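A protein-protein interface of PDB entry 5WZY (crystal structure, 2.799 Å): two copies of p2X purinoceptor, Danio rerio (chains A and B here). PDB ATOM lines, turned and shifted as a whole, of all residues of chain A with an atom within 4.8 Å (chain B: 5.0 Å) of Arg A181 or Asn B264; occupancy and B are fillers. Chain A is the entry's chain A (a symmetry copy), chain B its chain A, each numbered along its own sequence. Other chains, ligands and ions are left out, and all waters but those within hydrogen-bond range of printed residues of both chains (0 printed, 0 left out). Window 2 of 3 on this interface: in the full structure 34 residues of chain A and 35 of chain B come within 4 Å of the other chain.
The backbone NH (N) of Lys B260 lies close to the side-chain amide oxygen (OD1) of Asn A170, at 3.0 Å. NH2 of Arg A181 sits close to ND2 of Asn B264 (3.4 Å). The guanidinium group of Arg A181 sits at hydrogen-bond distance from the backbone carbonyl oxygen of Val B266 (2.8 Å). O of Ala B267 is in hydrogen-bond range of NZ of Lys A168 (3.0 Å). The backbone carbonyl oxygen (O) of Ala B267 is in hydrogen-bond range of the guanidinium group (NH1) of Arg A181.
The side-chain amide nitrogen (ND2) of Asn B264 sits close to the backbone carbonyl oxygen (O) of Asp B261 (3.4 Å).
Among the printed residues, pairs that only touch across the chains: Lys A180 with Lys B260, Arg A181 with Lys B260, Ile A183 with Val B266 and Ile A183 with Ala B267.
Of the printed residues of chain B, Arg A181 touches Lys B260, Asn B264, Val B266 and Ala B267. Asn B264 touches one residue of chain A. Of the printed residues of chain B, Asn A170 touches Lys B260 (3.0 Å). Of the printed residues of chain B, Lys A180 touches Lys B260. Of the printed residues of chain A, Val B266 touches Arg A181 and Ile A183. Of the printed residues of chain A, Lys B260 touches Asn A170 (3.0 Å), Lys A180 (3.4 Å) and Arg A181 (3.7 Å). Printed residues of chain B within 4 Å of Ile A183: Val B266 and Ala B267. Leu A184 touches none of the printed residues of chain B. The nearest residue of chain A that does not touch Asn B264 is Ile A183 (4.7 Å). The nearest printed residue of chain A that does not touch Val B266 is Lys A168 (5.9 Å).
Printed residues of chain B that touch a printed residue of chain A: Lys B260, Asn B264, Val B266 and Ala B267. Hydrophobic or aromatic side chains of chain B that line the printed part of chain A: Val B266 and Ala B267. Printed residues of chain A that touch a printed residue of chain B: Lys A168, Asn A170, Lys A180, Arg A181 and Ile A183. Hydrophobic or aromatic side chains of chain A that line the printed part of chain B: Ile A183. Among the printed residues, no Asp or Glu carboxylate lies within 4 Å of a Lys or Arg side-chain nitrogen of the other chain.
No position is printed for both chains. Of the 9 pairs that touch across the chains among the printed residues, none has its exchanged pair printed and touching as well.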
ATOM      1  N   LYS A 168       2.194   1.021 -28.217  1.00  0.00           N
ATOM      2  CA  LYS A 168       3.526   1.595 -28.333  1.00  0.00           C
ATOM      3  C   LYS A 168       3.630   2.521 -29.544  1.00  0.00           C
ATOM      4  O   LYS A 168       3.352   2.128 -30.670  1.00  0.00           O
ATOM      5  CB  LYS A 168       4.577   0.511 -28.414  1.00  0.00           C
ATOM      6  CG  LYS A 168       5.940   1.064 -28.195  1.00  0.00           C
ATOM      7  CD  LYS A 168       6.988   0.181 -28.813  1.00  0.00           C
ATOM      8  CE  LYS A 168       6.959  -1.197 -28.231  1.00  0.00           C
ATOM      9  NZ  LYS A 168       7.965  -1.995 -28.977  1.00  0.00           N
ATOM     10  N   ASN A 169       4.020   3.762 -29.298  1.00  0.00           N
ATOM     11  CA  ASN A 169       3.891   4.809 -30.297  1.00  0.00           C
ATOM     12  C   ASN A 169       5.160   5.627 -30.411  1.00  0.00           C
ATOM     13  O   ASN A 169       5.582   6.289 -29.463  1.00  0.00           O
ATOM     14  CB  ASN A 169       2.696   5.708 -29.962  1.00  0.00           C
ATOM     15  CG  ASN A 169       2.471   6.809 -30.988  1.00  0.00           C
ATOM     16  OD1 ASN A 169       1.934   7.867 -30.660  1.00  0.00           O
ATOM     17  ND2 ASN A 169       2.868   6.565 -32.234  1.00  0.00           N
ATOM     18  N   ASN A 170       5.760   5.562 -31.593  1.00  0.00           N
ATOM     19  CA  ASN A 170       6.901   6.389 -31.942  1.00  0.00           C
ATOM     20  C   ASN A 170       6.498   7.544 -32.835  1.00  0.00           C
ATOM     21  O   ASN A 170       5.944   7.340 -33.911  1.00  0.00           O
ATOM     22  CB  ASN A 170       7.941   5.546 -32.641  1.00  0.00           C
ATOM     23  CG  ASN A 170       8.744   4.727 -31.672  1.00  0.00           C
ATOM     24  OD1 ASN A 170       9.717   5.225 -31.108  1.00  0.00           O
ATOM     25  ND2 ASN A 170       8.342   3.468 -31.454  1.00  0.00           N
ATOM     26  N   ASN A 179      12.238  13.532 -31.835  1.00  0.00           N
ATOM     27  CA  ASN A 179      11.859  12.127 -31.762  1.00  0.00           C
ATOM     28  C   ASN A 179      11.435  11.752 -30.352  1.00  0.00           C
ATOM     29  O   ASN A 179      12.176  11.966 -29.402  1.00  0.00           O
ATOM     30  CB  ASN A 179      13.038  11.240 -32.159  1.00  0.00           C
ATOM     31  CG  ASN A 179      13.461  11.441 -33.592  1.00  0.00           C
ATOM     32  OD1 ASN A 179      12.627  11.471 -34.499  1.00  0.00           O
ATOM     33  ND2 ASN A 179      14.766  11.586 -33.809  1.00  0.00           N
ATOM     34  N   LYS A 180      10.250  11.176 -30.209  1.00  0.00           N
ATOM     35  CA  LYS A 180       9.817  10.744 -28.892  1.00  0.00           C
ATOM     36  C   LYS A 180       8.931   9.519 -29.001  1.00  0.00           C
ATOM     37  O   LYS A 180       8.407   9.215 -30.065  1.00  0.00           O
ATOM     38  CB  LYS A 180       9.084  11.874 -28.163  1.00  0.00           C
ATOM     39  CG  LYS A 180       9.092  11.729 -26.652  1.00  0.00           C
ATOM     40  CD  LYS A 180       8.588  12.985 -25.971  1.00  0.00           C
ATOM     41  CE  LYS A 180       8.642  12.832 -24.455  1.00  0.00           C
ATOM     42  NZ  LYS A 180       8.318  14.094 -23.749  1.00  0.00           N
ATOM     43  N   ARG A 181       8.774   8.825 -27.882  1.00  0.00           N
ATOM     44  CA  ARG A 181       7.992   7.607 -27.793  1.00  0.00           C
ATOM     45  C   ARG A 181       6.928   7.838 -26.718  1.00  0.00           C
ATOM     46  O   ARG A 181       7.122   8.671 -25.835  1.00  0.00           O
ATOM     47  CB  ARG A 181       8.939   6.484 -27.399  1.00  0.00           C
ATOM     48  CG  ARG A 181       8.467   5.116 -27.735  1.00  0.00           C
ATOM     49  CD  ARG A 181       9.656   4.219 -27.938  1.00  0.00           C
ATOM     50  NE  ARG A 181      10.438   4.086 -26.721  1.00  0.00           N
ATOM     51  CZ  ARG A 181      10.487   2.975 -25.999  1.00  0.00           C
ATOM     52  NH1 ARG A 181       9.800   1.913 -26.391  1.00  0.00           N
ATOM     53  NH2 ARG A 181      11.226   2.920 -24.895  1.00  0.00           N
ATOM     54  N   ASN A 182       5.798   7.135 -26.773  1.00  0.00           N
ATOM     55  CA  ASN A 182       4.744   7.390 -25.779  1.00  0.00           C
ATOM     56  C   ASN A 182       5.056   6.631 -24.502  1.00  0.00           C
ATOM     57  O   ASN A 182       4.343   6.715 -23.498  1.00  0.00           O
ATOM     58  CB  ASN A 182       3.329   7.096 -26.314  1.00  0.00           C
ATOM     59  CG  ASN A 182       3.010   5.619 -26.363  1.00  0.00           C
ATOM     60  OD1 ASN A 182       3.873   4.802 -26.631  1.00  0.00           O
ATOM     61  ND2 ASN A 182       1.762   5.273 -26.107  1.00  0.00           N
ATOM     62  N   ILE A 183       6.159   5.901 -24.567  1.00  0.00           N
ATOM     63  CA  ILE A 183       6.748   5.295 -23.401  1.00  0.00           C
ATOM     64  C   ILE A 183       7.736   6.351 -22.930  1.00  0.00           C
ATOM     65  O   ILE A 183       8.843   6.489 -23.467  1.00  0.00           O
ATOM     66  CB  ILE A 183       7.471   3.991 -23.817  1.00  0.00           C
ATOM     67  CG1 ILE A 183       6.434   2.970 -24.310  1.00  0.00           C
ATOM     68  CG2 ILE A 183       8.335   3.439 -22.695  1.00  0.00           C
ATOM     69  CD1 ILE A 183       6.956   1.567 -24.472  1.00  0.00           C
ATOM     70  N   LEU A 184       7.340   7.052 -21.870  1.00  0.00           N
ATOM     71  CA  LEU A 184       8.002   8.273 -21.436  1.00  0.00           C
ATOM     72  C   LEU A 184       9.256   7.958 -20.640  1.00  0.00           C
ATOM     73  O   LEU A 184       9.382   6.869 -20.081  1.00  0.00           O
ATOM     74  CB  LEU A 184       7.040   9.100 -20.590  1.00  0.00           C
ATOM     75  CG  LEU A 184       6.161  10.127 -21.304  1.00  0.00           C
ATOM     76  CD1 LEU A 184       6.186   9.951 -22.816  1.00  0.00           C
ATOM     77  CD2 LEU A 184       4.747  10.058 -20.771  1.00  0.00           C
ATOM     78  N   TRP A 237      -0.404  14.350 -30.184  1.00  0.00           N
ATOM     79  CA  TRP A 237       0.822  15.007 -29.747  1.00  0.00           C
ATOM     80  C   TRP A 237       0.898  16.442 -30.247  1.00  0.00           C
ATOM     81  O   TRP A 237       1.497  16.714 -31.284  1.00  0.00           O
ATOM     82  CB  TRP A 237       2.016  14.307 -30.374  1.00  0.00           C
ATOM     83  CG  TRP A 237       2.257  12.945 -29.923  1.00  0.00           C
ATOM     84  CD1 TRP A 237       1.620  11.822 -30.333  1.00  0.00           C
ATOM     85  CD2 TRP A 237       3.247  12.529 -28.985  1.00  0.00           C
ATOM     86  NE1 TRP A 237       2.144  10.722 -29.702  1.00  0.00           N
ATOM     87  CE2 TRP A 237       3.148  11.133 -28.868  1.00  0.00           C
ATOM     88  CE3 TRP A 237       4.207  13.205 -28.226  1.00  0.00           C
ATOM     89  CZ2 TRP A 237       3.970  10.397 -28.024  1.00  0.00           C
ATOM     90  CZ3 TRP A 237       5.023  12.477 -27.396  1.00  0.00           C
ATOM     91  CH2 TRP A 237       4.903  11.085 -27.301  1.00  0.00           C
ATOM     92  N   LYS B 260      12.711   5.498 -30.770  1.00  0.00           N
ATOM     93  CA  LYS B 260      12.794   6.959 -30.556  1.00  0.00           C
ATOM     94  C   LYS B 260      13.838   7.405 -29.510  1.00  0.00           C
ATOM     95  O   LYS B 260      14.586   8.368 -29.743  1.00  0.00           O
ATOM     96  CB  LYS B 260      11.419   7.547 -30.203  1.00  0.00           C
ATOM     97  N   ASP B 261      13.889   6.709 -28.369  1.00  0.00           N
ATOM     98  CA  ASP B 261      14.899   6.986 -27.333  1.00  0.00           C
ATOM     99  C   ASP B 261      15.834   5.780 -27.103  1.00  0.00           C
ATOM    100  O   ASP B 261      15.725   5.109 -26.073  1.00  0.00           O
ATOM    101  CB  ASP B 261      14.228   7.401 -26.010  1.00  0.00           C
ATOM    102  N   PRO B 262      16.779   5.534 -28.046  1.00  0.00           N
ATOM    103  CA  PRO B 262      17.635   4.332 -28.125  1.00  0.00           C
ATOM    104  C   PRO B 262      18.490   4.037 -26.882  1.00  0.00           C
ATOM    105  O   PRO B 262      19.084   2.957 -26.798  1.00  0.00           O
ATOM    106  CB  PRO B 262      18.519   4.592 -29.356  1.00  0.00           C
ATOM    107  CG  PRO B 262      18.426   6.058 -29.607  1.00  0.00           C
ATOM    108  CD  PRO B 262      17.059   6.466 -29.155  1.00  0.00           C
ATOM    109  N   ASP B 263      18.587   4.995 -25.963  1.00  0.00           N
ATOM    110  CA  ASP B 263      19.168   4.743 -24.641  1.00  0.00           C
ATOM    111  C   ASP B 263      18.316   3.744 -23.836  1.00  0.00           C
ATOM    112  O   ASP B 263      18.794   3.149 -22.857  1.00  0.00           O
ATOM    113  CB  ASP B 263      19.299   6.048 -23.839  1.00  0.00           C
ATOM    114  CG  ASP B 263      19.401   7.284 -24.722  1.00  0.00           C
ATOM    115  OD1 ASP B 263      19.413   7.141 -25.968  1.00  0.00           O
ATOM    116  OD2 ASP B 263      19.488   8.400 -24.161  1.00  0.00           O
ATOM    117  N   ASN B 264      17.055   3.584 -24.250  1.00  0.00           N
ATOM    118  CA  ASN B 264      16.083   2.749 -23.545  1.00  0.00           C
ATOM    119  C   ASN B 264      16.191   1.257 -23.828  1.00  0.00           C
ATOM    120  O   ASN B 264      16.312   0.827 -24.976  1.00  0.00           O
ATOM    121  CB  ASN B 264      14.648   3.204 -23.843  1.00  0.00           C
ATOM    122  CG  ASN B 264      14.261   4.468 -23.089  1.00  0.00           C
ATOM    123  OD1 ASN B 264      14.792   4.747 -22.009  1.00  0.00           O
ATOM    124  ND2 ASN B 264      13.327   5.238 -23.655  1.00  0.00           N
ATOM    125  N   ASN B 265      16.157   0.480 -22.753  1.00  0.00           N
ATOM    126  CA  ASN B 265      15.970  -0.962 -22.830  1.00  0.00           C
ATOM    127  C   ASN B 265      14.480  -1.284 -22.657  1.00  0.00           C
ATOM    128  O   ASN B 265      14.092  -2.447 -22.530  1.00  0.00           O
ATOM    129  CB  ASN B 265      16.816  -1.675 -21.764  1.00  0.00           C
ATOM    130  N   VAL B 266      13.652  -0.243 -22.613  1.00  0.00           N
ATOM    131  CA  VAL B 266      12.248  -0.418 -22.271  1.00  0.00           C
ATOM    132  C   VAL B 266      11.340  -0.690 -23.470  1.00  0.00           C
ATOM    133  O   VAL B 266      11.199   0.149 -24.361  1.00  0.00           O
ATOM    134  CB  VAL B 266      11.717   0.778 -21.486  1.00  0.00           C
ATOM    135  CG1 VAL B 266      10.197   0.678 -21.334  1.00  0.00           C
ATOM    136  CG2 VAL B 266      12.388   0.826 -20.137  1.00  0.00           C
ATOM    137  N   ALA B 267      10.719  -1.866 -23.457  1.00  0.00           N
ATOM    138  CA  ALA B 267       9.859  -2.332 -24.543  1.00  0.00           C
ATOM    139  C   ALA B 267      10.500  -2.196 -25.935  1.00  0.00           C
ATOM    140  O   ALA B 267       9.959  -1.526 -26.817  1.00  0.00           O
ATOM    141  CB  ALA B 267       8.489  -1.628 -24.487  1.00  0.00           C
